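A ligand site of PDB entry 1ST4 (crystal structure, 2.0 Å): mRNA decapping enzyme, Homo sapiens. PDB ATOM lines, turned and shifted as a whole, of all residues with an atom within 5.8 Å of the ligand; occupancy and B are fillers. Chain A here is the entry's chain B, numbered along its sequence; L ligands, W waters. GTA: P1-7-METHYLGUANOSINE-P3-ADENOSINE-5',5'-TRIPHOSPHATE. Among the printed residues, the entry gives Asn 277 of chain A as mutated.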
ATOM      1  N   LEU A 144     -33.714  28.122 -16.091  1.00  0.00           N
ATOM      2  CA  LEU A 144     -35.087  27.908 -16.531  1.00  0.00           C
ATOM      3  C   LEU A 144     -35.225  26.797 -17.589  1.00  0.00           C
ATOM      4  O   LEU A 144     -34.473  26.755 -18.621  1.00  0.00           O
ATOM      5  CB  LEU A 144     -35.788  29.219 -16.983  1.00  0.00           C
ATOM      6  CG  LEU A 144     -37.246  28.955 -17.473  1.00  0.00           C
ATOM      7  CD1 LEU A 144     -38.087  28.853 -16.252  1.00  0.00           C
ATOM      8  CD2 LEU A 144     -37.677  30.079 -18.384  1.00  0.00           C
ATOM      9  N   ARG A 145     -36.139  25.877 -17.286  1.00  0.00           N
ATOM     10  CA  ARG A 145     -36.530  24.777 -18.187  1.00  0.00           C
ATOM     11  C   ARG A 145     -38.063  24.718 -18.226  1.00  0.00           C
ATOM     12  O   ARG A 145     -38.709  24.861 -17.180  1.00  0.00           O
ATOM     13  CB  ARG A 145     -35.977  23.386 -17.743  1.00  0.00           C
ATOM     14  CG  ARG A 145     -34.396  23.205 -17.923  1.00  0.00           C
ATOM     15  CD  ARG A 145     -33.985  23.184 -19.373  1.00  0.00           C
ATOM     16  NE  ARG A 145     -32.640  22.716 -19.631  1.00  0.00           N
ATOM     17  CZ  ARG A 145     -32.334  21.673 -20.438  1.00  0.00           C
ATOM     18  NH1 ARG A 145     -33.305  20.959 -21.052  1.00  0.00           N
ATOM     19  NH2 ARG A 145     -31.061  21.329 -20.630  1.00  0.00           N
ATOM     20  N   GLN A 146     -38.597  24.493 -19.414  1.00  0.00           N
ATOM     21  CA  GLN A 146     -40.062  24.326 -19.622  1.00  0.00           C
ATOM     22  C   GLN A 146     -40.446  22.867 -19.260  1.00  0.00           C
ATOM     23  O   GLN A 146     -39.711  21.967 -19.569  1.00  0.00           O
ATOM     24  CB  GLN A 146     -40.301  24.518 -21.126  1.00  0.00           C
ATOM     25  CG  GLN A 146     -39.946  25.994 -21.594  1.00  0.00           C
ATOM     26  CD  GLN A 146     -40.657  27.043 -20.771  1.00  0.00           C
ATOM     27  OE1 GLN A 146     -41.841  26.881 -20.462  1.00  0.00           O
ATOM     28  NE2 GLN A 146     -39.934  28.099 -20.339  1.00  0.00           N
ATOM     29  N   ASP A 147     -41.576  22.688 -18.638  1.00  0.00           N
ATOM     30  CA  ASP A 147     -42.232  21.363 -18.465  1.00  0.00           C
ATOM     31  C   ASP A 147     -42.730  20.855 -19.807  1.00  0.00           C
ATOM     32  O   ASP A 147     -42.890  21.658 -20.743  1.00  0.00           O
ATOM     33  CB  ASP A 147     -43.435  21.585 -17.574  1.00  0.00           C
ATOM     34  CG  ASP A 147     -43.060  21.718 -16.111  1.00  0.00           C
ATOM     35  OD1 ASP A 147     -43.910  22.267 -15.298  1.00  0.00           O
ATOM     36  OD2 ASP A 147     -41.926  21.265 -15.757  1.00  0.00           O
ATOM     37  N   LEU A 148     -42.877  19.539 -19.915  1.00  0.00           N
ATOM     38  CA  LEU A 148     -43.114  18.929 -21.180  1.00  0.00           C
ATOM     39  C   LEU A 148     -44.540  18.396 -21.218  1.00  0.00           C
ATOM     40  O   LEU A 148     -45.155  18.112 -20.159  1.00  0.00           O
ATOM     41  CB  LEU A 148     -42.101  17.794 -21.425  1.00  0.00           C
ATOM     42  CG  LEU A 148     -40.624  18.164 -21.552  1.00  0.00           C
ATOM     43  CD1 LEU A 148     -39.987  16.883 -21.999  1.00  0.00           C
ATOM     44  CD2 LEU A 148     -40.337  19.393 -22.547  1.00  0.00           C
ATOM     45  N   LEU A 171     -35.353  26.865 -36.092  1.00  0.00           N
ATOM     46  CA  LEU A 171     -34.007  27.373 -35.712  1.00  0.00           C
ATOM     47  C   LEU A 171     -33.002  27.168 -36.847  1.00  0.00           C
ATOM     48  O   LEU A 171     -33.095  26.182 -37.611  1.00  0.00           O
ATOM     49  CB  LEU A 171     -33.439  26.761 -34.423  1.00  0.00           C
ATOM     50  CG  LEU A 171     -34.239  26.264 -33.227  1.00  0.00           C
ATOM     51  CD1 LEU A 171     -35.284  25.150 -33.623  1.00  0.00           C
ATOM     52  CD2 LEU A 171     -33.284  25.807 -32.070  1.00  0.00           C
ATOM     53  N   TRP A 175     -25.052  26.298 -38.702  1.00  0.00           N
ATOM     54  CA  TRP A 175     -23.928  25.589 -38.022  1.00  0.00           C
ATOM     55  C   TRP A 175     -23.634  24.232 -38.680  1.00  0.00           C
ATOM     56  O   TRP A 175     -22.488  23.858 -38.736  1.00  0.00           O
ATOM     57  CB  TRP A 175     -24.128  25.444 -36.485  1.00  0.00           C
ATOM     58  CG  TRP A 175     -25.268  24.470 -36.195  1.00  0.00           C
ATOM     59  CD1 TRP A 175     -26.602  24.758 -36.218  1.00  0.00           C
ATOM     60  CD2 TRP A 175     -25.168  23.070 -35.952  1.00  0.00           C
ATOM     61  NE1 TRP A 175     -27.324  23.616 -35.966  1.00  0.00           N
ATOM     62  CE2 TRP A 175     -26.468  22.569 -35.802  1.00  0.00           C
ATOM     63  CE3 TRP A 175     -24.087  22.179 -35.813  1.00  0.00           C
ATOM     64  CZ2 TRP A 175     -26.727  21.221 -35.514  1.00  0.00           C
ATOM     65  CZ3 TRP A 175     -24.360  20.826 -35.544  1.00  0.00           C
ATOM     66  CH2 TRP A 175     -25.656  20.376 -35.418  1.00  0.00           C
ATOM     67  N   ILE A 179     -20.173  23.124 -40.927  1.00  0.00           N
ATOM     68  CA  ILE A 179     -19.440  21.862 -40.889  1.00  0.00           C
ATOM     69  C   ILE A 179     -19.331  21.186 -42.237  1.00  0.00           C
ATOM     70  O   ILE A 179     -18.216  20.827 -42.629  1.00  0.00           O
ATOM     71  CB  ILE A 179     -20.048  20.890 -39.833  1.00  0.00           C
ATOM     72  CG1 ILE A 179     -19.814  21.438 -38.410  1.00  0.00           C
ATOM     73  CG2 ILE A 179     -19.481  19.458 -40.006  1.00  0.00           C
ATOM     74  CD1 ILE A 179     -20.805  20.841 -37.387  1.00  0.00           C
ATOM     75  N   GLU A 185     -15.243  23.619 -37.469  1.00  0.00           N
ATOM     76  CA  GLU A 185     -15.004  22.339 -36.789  1.00  0.00           C
ATOM     77  C   GLU A 185     -14.215  21.292 -37.649  1.00  0.00           C
ATOM     78  O   GLU A 185     -14.414  20.053 -37.547  1.00  0.00           O
ATOM     79  CB  GLU A 185     -16.344  21.735 -36.300  1.00  0.00           C
ATOM     80  CG  GLU A 185     -17.117  22.551 -35.248  1.00  0.00           C
ATOM     81  CD  GLU A 185     -18.454  21.909 -34.855  1.00  0.00           C
ATOM     82  OE1 GLU A 185     -19.542  22.533 -35.106  1.00  0.00           O
ATOM     83  OE2 GLU A 185     -18.410  20.756 -34.328  1.00  0.00           O
ATOM     84  N   ARG A 188     -11.870  18.827 -35.902  1.00  0.00           N
ATOM     85  CA  ARG A 188     -12.515  17.818 -35.027  1.00  0.00           C
ATOM     86  C   ARG A 188     -13.249  16.722 -35.755  1.00  0.00           C
ATOM     87  O   ARG A 188     -13.925  15.937 -35.091  1.00  0.00           O
ATOM     88  CB  ARG A 188     -13.546  18.428 -34.064  1.00  0.00           C
ATOM     89  CG  ARG A 188     -13.183  19.704 -33.334  1.00  0.00           C
ATOM     90  CD  ARG A 188     -14.366  20.610 -33.203  1.00  0.00           C
ATOM     91  NE  ARG A 188     -14.742  20.721 -31.793  1.00  0.00           N
ATOM     92  CZ  ARG A 188     -15.828  20.144 -31.229  1.00  0.00           C
ATOM     93  NH1 ARG A 188     -16.709  19.439 -31.946  1.00  0.00           N
ATOM     94  NH2 ARG A 188     -16.033  20.326 -29.938  1.00  0.00           N
ATOM     95  N   ILE A 203     -18.840  14.162 -36.085  1.00  0.00           N
ATOM     96  CA  ILE A 203     -18.055  15.042 -35.233  1.00  0.00           C
ATOM     97  C   ILE A 203     -18.558  14.800 -33.818  1.00  0.00           C
ATOM     98  O   ILE A 203     -19.676  14.312 -33.609  1.00  0.00           O
ATOM     99  CB  ILE A 203     -18.265  16.652 -35.540  1.00  0.00           C
ATOM    100  CG1 ILE A 203     -19.709  17.087 -35.884  1.00  0.00           C
ATOM    101  CG2 ILE A 203     -17.178  17.312 -36.497  1.00  0.00           C
ATOM    102  CD1 ILE A 203     -20.585  16.080 -36.626  1.00  0.00           C
ATOM    103  N   PRO A 204     -17.726  15.144 -32.853  1.00  0.00           N
ATOM    104  CA  PRO A 204     -18.182  15.145 -31.474  1.00  0.00           C
ATOM    105  C   PRO A 204     -19.329  16.105 -31.359  1.00  0.00           C
ATOM    106  O   PRO A 204     -19.336  17.178 -31.999  1.00  0.00           O
ATOM    107  CB  PRO A 204     -16.990  15.680 -30.690  1.00  0.00           C
ATOM    108  CG  PRO A 204     -15.790  15.662 -31.649  1.00  0.00           C
ATOM    109  CD  PRO A 204     -16.308  15.486 -33.008  1.00  0.00           C
ATOM    110  N   ASP A 205     -20.313  15.720 -30.557  1.00  0.00           N
ATOM    111  CA  ASP A 205     -21.368  16.627 -30.252  1.00  0.00           C
ATOM    112  C   ASP A 205     -20.805  17.676 -29.291  1.00  0.00           C
ATOM    113  O   ASP A 205     -19.938  17.341 -28.496  1.00  0.00           O
ATOM    114  CB  ASP A 205     -22.487  15.812 -29.633  1.00  0.00           C
ATOM    115  CG  ASP A 205     -23.674  16.637 -29.398  1.00  0.00           C
ATOM    116  OD1 ASP A 205     -23.629  17.499 -28.486  1.00  0.00           O
ATOM    117  OD2 ASP A 205     -24.700  16.414 -30.069  1.00  0.00           O
ATOM    118  N   LEU A 206     -21.297  18.928 -29.313  1.00  0.00           N
ATOM    119  CA  LEU A 206     -20.833  19.945 -28.309  1.00  0.00           C
ATOM    120  C   LEU A 206     -21.053  19.520 -26.828  1.00  0.00           C
ATOM    121  O   LEU A 206     -20.462  20.080 -25.900  1.00  0.00           O
ATOM    122  CB  LEU A 206     -21.448  21.364 -28.534  1.00  0.00           C
ATOM    123  CG  LEU A 206     -21.000  22.273 -29.741  1.00  0.00           C
ATOM    124  CD1 LEU A 206     -20.914  23.788 -29.411  1.00  0.00           C
ATOM    125  CD2 LEU A 206     -19.633  21.838 -30.367  1.00  0.00           C
ATOM    126  N   LYS A 207     -21.933  18.531 -26.617  1.00  0.00           N
ATOM    127  CA  LYS A 207     -22.261  18.107 -25.275  1.00  0.00           C
ATOM    128  C   LYS A 207     -21.105  17.383 -24.559  1.00  0.00           C
ATOM    129  O   LYS A 207     -21.108  17.273 -23.296  1.00  0.00           O
ATOM    130  CB  LYS A 207     -23.567  17.286 -25.271  1.00  0.00           C
ATOM    131  CG  LYS A 207     -24.924  18.096 -25.387  1.00  0.00           C
ATOM    132  CD  LYS A 207     -26.061  17.155 -25.861  1.00  0.00           C
ATOM    133  CE  LYS A 207     -27.300  17.850 -26.427  1.00  0.00           C
ATOM    134  NZ  LYS A 207     -28.284  16.919 -27.123  1.00  0.00           N
ATOM    135  N   TYR A 217     -20.259  11.064 -26.805  1.00  0.00           N
ATOM    136  CA  TYR A 217     -21.434  11.481 -27.629  1.00  0.00           C
ATOM    137  C   TYR A 217     -21.006  12.064 -29.002  1.00  0.00           C
ATOM    138  O   TYR A 217     -20.278  13.092 -29.040  1.00  0.00           O
ATOM    139  CB  TYR A 217     -22.158  12.585 -26.829  1.00  0.00           C
ATOM    140  CG  TYR A 217     -23.637  12.842 -27.207  1.00  0.00           C
ATOM    141  CD1 TYR A 217     -24.054  12.859 -28.533  1.00  0.00           C
ATOM    142  CD2 TYR A 217     -24.615  13.067 -26.193  1.00  0.00           C
ATOM    143  CE1 TYR A 217     -25.368  13.075 -28.848  1.00  0.00           C
ATOM    144  CE2 TYR A 217     -25.903  13.326 -26.516  1.00  0.00           C
ATOM    145  CZ  TYR A 217     -26.304  13.296 -27.807  1.00  0.00           C
ATOM    146  OH  TYR A 217     -27.618  13.507 -28.085  1.00  0.00           O
ATOM    147  N   ILE A 219     -22.420  13.334 -33.128  1.00  0.00           N
ATOM    148  CA  ILE A 219     -23.487  13.396 -34.164  1.00  0.00           C
ATOM    149  C   ILE A 219     -23.007  13.181 -35.627  1.00  0.00           C
ATOM    150  O   ILE A 219     -21.933  13.594 -36.034  1.00  0.00           O
ATOM    151  CB  ILE A 219     -24.482  14.683 -34.104  1.00  0.00           C
ATOM    152  CG1 ILE A 219     -23.801  16.018 -34.025  1.00  0.00           C
ATOM    153  CG2 ILE A 219     -25.573  14.608 -32.994  1.00  0.00           C
ATOM    154  CD1 ILE A 219     -22.468  15.992 -33.365  1.00  0.00           C
ATOM    155  N   HIS A 268     -33.421  11.724 -32.868  1.00  0.00           N
ATOM    156  CA  HIS A 268     -34.574  12.388 -32.233  1.00  0.00           C
ATOM    157  C   HIS A 268     -35.814  12.666 -33.108  1.00  0.00           C
ATOM    158  O   HIS A 268     -35.714  13.063 -34.294  1.00  0.00           O
ATOM    159  CB  HIS A 268     -34.128  13.673 -31.623  1.00  0.00           C
ATOM    160  CG  HIS A 268     -33.120  13.499 -30.545  1.00  0.00           C
ATOM    161  ND1 HIS A 268     -32.156  14.436 -30.283  1.00  0.00           N
ATOM    162  CD2 HIS A 268     -32.942  12.494 -29.640  1.00  0.00           C
ATOM    163  CE1 HIS A 268     -31.405  14.020 -29.272  1.00  0.00           C
ATOM    164  NE2 HIS A 268     -31.875  12.868 -28.853  1.00  0.00           N
ATOM    165  N   LEU A 270     -39.265  14.842 -31.825  1.00  0.00           N
ATOM    166  CA  LEU A 270     -38.892  15.888 -32.803  1.00  0.00           C
ATOM    167  C   LEU A 270     -37.445  16.356 -32.626  1.00  0.00           C
ATOM    168  O   LEU A 270     -36.994  16.570 -31.462  1.00  0.00           O
ATOM    169  CB  LEU A 270     -39.809  17.043 -32.457  1.00  0.00           C
ATOM    170  CG  LEU A 270     -40.713  17.734 -33.442  1.00  0.00           C
ATOM    171  CD1 LEU A 270     -41.446  16.816 -34.385  1.00  0.00           C
ATOM    172  CD2 LEU A 270     -41.671  18.606 -32.661  1.00  0.00           C
ATOM    173  N   PRO A 271     -36.655  16.546 -33.686  1.00  0.00           N
ATOM    174  CA  PRO A 271     -35.320  17.114 -33.460  1.00  0.00           C
ATOM    175  C   PRO A 271     -35.371  18.578 -33.116  1.00  0.00           C
ATOM    176  O   PRO A 271     -36.310  19.218 -33.412  1.00  0.00           O
ATOM    177  CB  PRO A 271     -34.644  16.984 -34.827  1.00  0.00           C
ATOM    178  CG  PRO A 271     -35.694  17.103 -35.724  1.00  0.00           C
ATOM    179  CD  PRO A 271     -36.892  16.326 -35.127  1.00  0.00           C
ATOM    180  N   SER A 272     -34.319  19.141 -32.580  1.00  0.00           N
ATOM    181  CA  SER A 272     -34.312  20.594 -32.533  1.00  0.00           C
ATOM    182  C   SER A 272     -33.946  21.244 -33.865  1.00  0.00           C
ATOM    183  O   SER A 272     -34.470  22.337 -34.188  1.00  0.00           O
ATOM    184  CB  SER A 272     -33.342  21.162 -31.460  1.00  0.00           C
ATOM    185  OG  SER A 272     -33.890  20.947 -30.187  1.00  0.00           O
ATOM    186  N   TYR A 273     -32.992  20.631 -34.586  1.00  0.00           N
ATOM    187  CA  TYR A 273     -32.546  21.154 -35.883  1.00  0.00           C
ATOM    188  C   TYR A 273     -33.065  20.258 -37.002  1.00  0.00           C
ATOM    189  O   TYR A 273     -32.858  18.991 -37.005  1.00  0.00           O
ATOM    190  CB  TYR A 273     -31.051  21.266 -35.894  1.00  0.00           C
ATOM    191  CG  TYR A 273     -30.557  22.140 -34.773  1.00  0.00           C
ATOM    192  CD1 TYR A 273     -30.200  21.592 -33.533  1.00  0.00           C
ATOM    193  CD2 TYR A 273     -30.428  23.524 -34.933  1.00  0.00           C
ATOM    194  CE1 TYR A 273     -29.718  22.382 -32.492  1.00  0.00           C
ATOM    195  CE2 TYR A 273     -29.987  24.336 -33.887  1.00  0.00           C
ATOM    196  CZ  TYR A 273     -29.645  23.762 -32.662  1.00  0.00           C
ATOM    197  OH  TYR A 273     -29.189  24.567 -31.641  1.00  0.00           O
ATOM    198  N   TYR A 274     -33.751  20.903 -37.951  1.00  0.00           N
ATOM    199  CA  TYR A 274     -34.363  20.129 -39.039  1.00  0.00           C
ATOM    200  C   TYR A 274     -33.496  19.753 -40.272  1.00  0.00           C
ATOM    201  O   TYR A 274     -33.887  19.961 -41.417  1.00  0.00           O
ATOM    202  CB  TYR A 274     -35.675  20.807 -39.441  1.00  0.00           C
ATOM    203  CG  TYR A 274     -36.697  20.649 -38.363  1.00  0.00           C
ATOM    204  CD1 TYR A 274     -36.792  21.572 -37.335  1.00  0.00           C
ATOM    205  CD2 TYR A 274     -37.523  19.531 -38.348  1.00  0.00           C
ATOM    206  CE1 TYR A 274     -37.730  21.398 -36.310  1.00  0.00           C
ATOM    207  CE2 TYR A 274     -38.467  19.362 -37.376  1.00  0.00           C
ATOM    208  CZ  TYR A 274     -38.569  20.303 -36.357  1.00  0.00           C
ATOM    209  OH  TYR A 274     -39.482  20.117 -35.374  1.00  0.00           O
ATOM    210  N   ASN A 277     -30.053  14.210 -38.378  1.00  0.00           N
ATOM    211  CA  ASN A 277     -28.810  14.096 -37.582  1.00  0.00           C
ATOM    212  C   ASN A 277     -28.878  12.858 -36.667  1.00  0.00           C
ATOM    213  O   ASN A 277     -29.931  12.563 -36.075  1.00  0.00           O
ATOM    214  CB  ASN A 277     -28.411  15.396 -36.884  1.00  0.00           C
ATOM    215  CG  ASN A 277     -29.488  15.897 -35.884  1.00  0.00           C
ATOM    216  OD1 ASN A 277     -29.586  15.379 -34.724  1.00  0.00           O
ATOM    217  ND2 ASN A 277     -30.329  16.852 -36.326  1.00  0.00           N
ATOM    218  N   HIS A 279     -27.549  10.270 -33.643  1.00  0.00           N
ATOM    219  CA  HIS A 279     -26.823  10.461 -32.378  1.00  0.00           C
ATOM    220  C   HIS A 279     -26.141   9.153 -31.974  1.00  0.00           C
ATOM    221  O   HIS A 279     -26.799   8.088 -32.016  1.00  0.00           O
ATOM    222  CB  HIS A 279     -27.781  10.929 -31.309  1.00  0.00           C
ATOM    223  CG  HIS A 279     -28.339  12.283 -31.566  1.00  0.00           C
ATOM    224  ND1 HIS A 279     -28.102  13.353 -30.737  1.00  0.00           N
ATOM    225  CD2 HIS A 279     -29.085  12.754 -32.613  1.00  0.00           C
ATOM    226  CE1 HIS A 279     -28.722  14.412 -31.229  1.00  0.00           C
ATOM    227  NE2 HIS A 279     -29.335  14.068 -32.348  1.00  0.00           N
ATOM    228  N   ARG A 294     -38.651  10.065 -27.125  1.00  0.00           N
ATOM    229  CA  ARG A 294     -37.933  10.849 -28.123  1.00  0.00           C
ATOM    230  C   ARG A 294     -37.013  10.127 -29.160  1.00  0.00           C
ATOM    231  O   ARG A 294     -36.827  10.650 -30.267  1.00  0.00           O
ATOM    232  CB  ARG A 294     -37.076  11.869 -27.385  1.00  0.00           C
ATOM    233  CG  ARG A 294     -37.022  13.095 -28.220  1.00  0.00           C
ATOM    234  CD  ARG A 294     -36.116  14.148 -27.736  1.00  0.00           C
ATOM    235  NE  ARG A 294     -36.032  15.203 -28.736  1.00  0.00           N
ATOM    236  CZ  ARG A 294     -35.050  16.071 -28.733  1.00  0.00           C
ATOM    237  NH1 ARG A 294     -34.122  15.998 -27.742  1.00  0.00           N
ATOM    238  NH2 ARG A 294     -34.988  17.001 -29.700  1.00  0.00           N
ATOM    239  N   ARG A 322     -42.304  21.261 -25.297  1.00  0.00           N
ATOM    240  CA  ARG A 322     -42.383  22.270 -24.259  1.00  0.00           C
ATOM    241  C   ARG A 322     -43.741  22.888 -24.049  1.00  0.00           C
ATOM    242  O   ARG A 322     -44.457  23.199 -25.011  1.00  0.00           O
ATOM    243  CB  ARG A 322     -41.433  23.425 -24.532  1.00  0.00           C
ATOM    244  CG  ARG A 322     -40.017  22.974 -24.656  1.00  0.00           C
ATOM    245  CD  ARG A 322     -39.051  24.217 -24.775  1.00  0.00           C
ATOM    246  NE  ARG A 322     -37.919  23.703 -25.499  1.00  0.00           N
ATOM    247  CZ  ARG A 322     -36.835  24.421 -25.861  1.00  0.00           C
ATOM    248  NH1 ARG A 322     -36.724  25.718 -25.553  1.00  0.00           N
ATOM    249  NH2 ARG A 322     -35.873  23.788 -26.512  1.00  0.00           N
HETATM  250  N2  GTA L   1     -20.666  19.698 -33.385  1.00  0.00           N
HETATM  251  O6  GTA L   1     -22.387  23.943 -33.358  1.00  0.00           O
HETATM  252  C6  GTA L   1     -22.566  22.731 -33.106  1.00  0.00           C
HETATM  253  C5  GTA L   1     -23.781  22.295 -32.515  1.00  0.00           C
HETATM  254  N7  GTA L   1     -24.923  22.870 -32.126  1.00  0.00           N
HETATM  255  C7  GTA L   1     -25.228  24.315 -32.254  1.00  0.00           C
HETATM  256  C8  GTA L   1     -25.714  21.881 -31.620  1.00  0.00           C
HETATM  257  N9  GTA L   1     -25.105  20.659 -31.680  1.00  0.00           N
HETATM  258  C4  GTA L   1     -23.911  20.934 -32.241  1.00  0.00           C
HETATM  259  N3  GTA L   1     -22.842  19.994 -32.529  1.00  0.00           N
HETATM  260  C2  GTA L   1     -21.712  20.504 -33.095  1.00  0.00           C
HETATM  261  N1  GTA L   1     -21.580  21.834 -33.384  1.00  0.00           N
HETATM  262  O3A GTA L   1     -27.358  16.736 -29.872  1.00  0.00           O
HETATM  263  C1A GTA L   1     -25.606  19.318 -31.252  1.00  0.00           C
HETATM  264  C2A GTA L   1     -26.566  19.207 -30.066  1.00  0.00           C
HETATM  265  C3A GTA L   1     -27.545  18.052 -30.434  1.00  0.00           C
HETATM  266  C4A GTA L   1     -27.385  17.922 -31.934  1.00  0.00           C
HETATM  267  C5A GTA L   1     -28.672  18.275 -32.605  1.00  0.00           C
HETATM  268  O4A GTA L   1     -26.414  18.854 -32.327  1.00  0.00           O
HETATM  269  O2A GTA L   1     -25.899  19.163 -28.809  1.00  0.00           O
HETATM  270  P1  GTA L   1     -31.129  17.433 -32.466  1.00  0.00           P
HETATM  271  O11 GTA L   1     -31.960  16.213 -32.548  1.00  0.00           O
HETATM  272  O12 GTA L   1     -31.502  18.300 -33.681  1.00  0.00           O
HETATM  273  O13 GTA L   1     -31.452  18.453 -31.232  1.00  0.00           O
HETATM  274  O15 GTA L   1     -29.555  17.216 -32.341  1.00  0.00           O
HETATM  275  P2  GTA L   1     -31.591  18.338 -29.617  1.00  0.00           P
HETATM  276  O22 GTA L   1     -30.724  17.149 -29.205  1.00  0.00           O
HETATM  277  O21 GTA L   1     -33.068  18.460 -29.382  1.00  0.00           O
HETATM  278  O23 GTA L   1     -30.593  19.583 -29.370  1.00  0.00           O
HETATM  279  P3  GTA L   1     -30.174  20.222 -28.014  1.00  0.00           P
HETATM  280  O32 GTA L   1     -29.017  21.141 -28.171  1.00  0.00           O
HETATM  281  O31 GTA L   1     -29.975  19.218 -26.893  1.00  0.00           O
HETATM  282  O33 GTA L   1     -31.596  21.036 -27.955  1.00  0.00           O
HETATM  283  C5B GTA L   1     -31.651  22.480 -28.219  1.00  0.00           C
HETATM  284  C4B GTA L   1     -31.733  23.385 -27.192  1.00  0.00           C
HETATM  285  O4B GTA L   1     -33.003  23.586 -26.468  1.00  0.00           O
HETATM  286  C3B GTA L   1     -30.616  23.465 -26.224  1.00  0.00           C
HETATM  287  O3B GTA L   1     -30.244  24.829 -26.207  1.00  0.00           O
HETATM  288  C2B GTA L   1     -31.324  23.002 -24.969  1.00  0.00           C
HETATM  289  O2B GTA L   1     -30.575  23.197 -23.763  1.00  0.00           O
HETATM  290  C1B GTA L   1     -32.693  23.677 -25.057  1.00  0.00           C
HETATM  291  N9C GTA L   1     -33.744  22.978 -24.271  1.00  0.00           N
HETATM  292  C8C GTA L   1     -33.951  21.525 -24.475  1.00  0.00           C
HETATM  293  N7C GTA L   1     -35.085  21.249 -23.577  1.00  0.00           N
HETATM  294  C5C GTA L   1     -35.506  22.389 -22.975  1.00  0.00           C
HETATM  295  C6C GTA L   1     -36.533  22.550 -22.045  1.00  0.00           C
HETATM  296  N6C GTA L   1     -37.207  21.543 -21.668  1.00  0.00           N
HETATM  297  N1C GTA L   1     -36.776  23.824 -21.561  1.00  0.00           N
HETATM  298  C2C GTA L   1     -35.990  24.866 -21.987  1.00  0.00           C
HETATM  299  N3C GTA L   1     -34.978  24.675 -22.894  1.00  0.00           N
HETATM  300  C4C GTA L   1     -34.721  23.446 -23.393  1.00  0.00           C
HETATM  301  O   HOH W   1     -34.564  18.738 -26.632  1.00  0.00           O
HETATM  302  O   HOH W   2     -32.052  13.727 -34.602  1.00  0.00           O
HETATM  303  O   HOH W   3     -36.610  18.694 -23.590  1.00  0.00           O
HETATM  304  O   HOH W   4     -20.381  24.977 -35.658  1.00  0.00           O
HETATM  305  O   HOH W   5     -24.873  21.259 -27.680  1.00  0.00           O
HETATM  306  O   HOH W   6     -28.008  23.448 -29.149  1.00  0.00           O
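The guanidinium group (NH2) of Arg 294 is in salt-bridge range of an oxygen (O21) of the ligand (2.4 Å).
N2 of the ligand lies within hydrogen-bond range of OE2 of Glu 185 (2.7 Å).
OD2 of Asp 205 is in hydrogen-bond range of O3A of the ligand.
An oxygen (O12) of the ligand is in hydrogen-bond range of the backbone NH of Ser 272 (3.1 Å).
An oxygen (O21) of the ligand sits at hydrogen-bond distance from the side-chain hydroxyl (OG) of Ser 272.
NZ of Lys 207 lies within salt-bridge range of O31 of the ligand, 2.9 Å away.
NH2 of Arg 322 lies within hydrogen-bond range of O4B of the ligand (2.9 Å).
O11 of the ligand lies within hydrogen-bond range of ND1 of His 268, at 2.9 Å.
A nitrogen (N1C) of the ligand is in hydrogen-bond range of the backbone NH (N) of Gln 146 (2.9 Å).
N6C of the ligand lies within hydrogen-bond range of O of Gln 146, 3.3 Å away.
O12 of the ligand is in hydrogen-bond range of N of Tyr 273 (2.9 Å).
O15 of the ligand lies close to OD1 of Asn 277 (3.0 Å).
An oxygen (O15) of the ligand lies close to a ring nitrogen (NE2) of His 279 (3.2 Å).
NH1 of Arg 145 is in hydrogen-bond range of N7C of the ligand (3.1 Å).
N2 of the ligand sits at hydrogen-bond distance from O of Pro 204 (3.2 Å).
The guanidinium group (NH2) of Arg 294 is in hydrogen-bond range of the backbone carbonyl oxygen (O) of Leu 270, at 2.7 Å.
NH1 of Arg 188 is in salt-bridge range of OE2 of Glu 185, at 3.2 Å.
O of Tyr 217 lies within hydrogen-bond range of N of Asp 205, 3.0 Å away.
The backbone carbonyl oxygen (O) of Tyr 273 is in hydrogen-bond range of the side-chain amide nitrogen (ND2) of Asn 277.
The side-chain amide oxygen of Asn 277 lies within hydrogen-bond range of a ring nitrogen (NE2) of His 279, at 2.7 Å.
The side-chain hydroxyl (OH) of Tyr 217 lies within hydrogen-bond range of a ring nitrogen (ND1) of His 279 (2.7 Å).
The backbone carbonyl oxygen (O) of Pro 204 lies within hydrogen-bond range of the guanidinium group (NH1) of Arg 188 (3.5 Å).
The backbone carbonyl oxygen (O) of Ile 203 lies within hydrogen-bond range of the backbone NH (N) of Ile 219, 3.0 Å away.
Residues that only touch the ligand: Trp 175, Leu 206, Pro 271, Tyr 217, Ile 203, Leu 148 and Ile 219.
Hydrophobic or aromatic side chains within 4 Å of the ligand: Leu 148, Trp 175, Ile 203, Leu 206, Ile 219, His 268, Pro 271, Tyr 273 and His 279.
The nearest printed residue that does not touch the ligand is Leu 144 (4.1 Å).
Water W6 bridges O32 of the ligand (2.7 Å) and OH of Tyr 273 (3.0 Å).
Water W1 bridges the guanidinium group (NH1) of Arg 294 and an oxygen (O21) of the ligand.
Water W4 bridges the side-chain carboxylate (OE1) of Glu 185 (2.6 Å) and an oxygen (O6) of the ligand (3.2 Å).
Water W2 lies within hydrogen-bond range of O of Asn 277, N of His 268 and O11 of the ligand.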
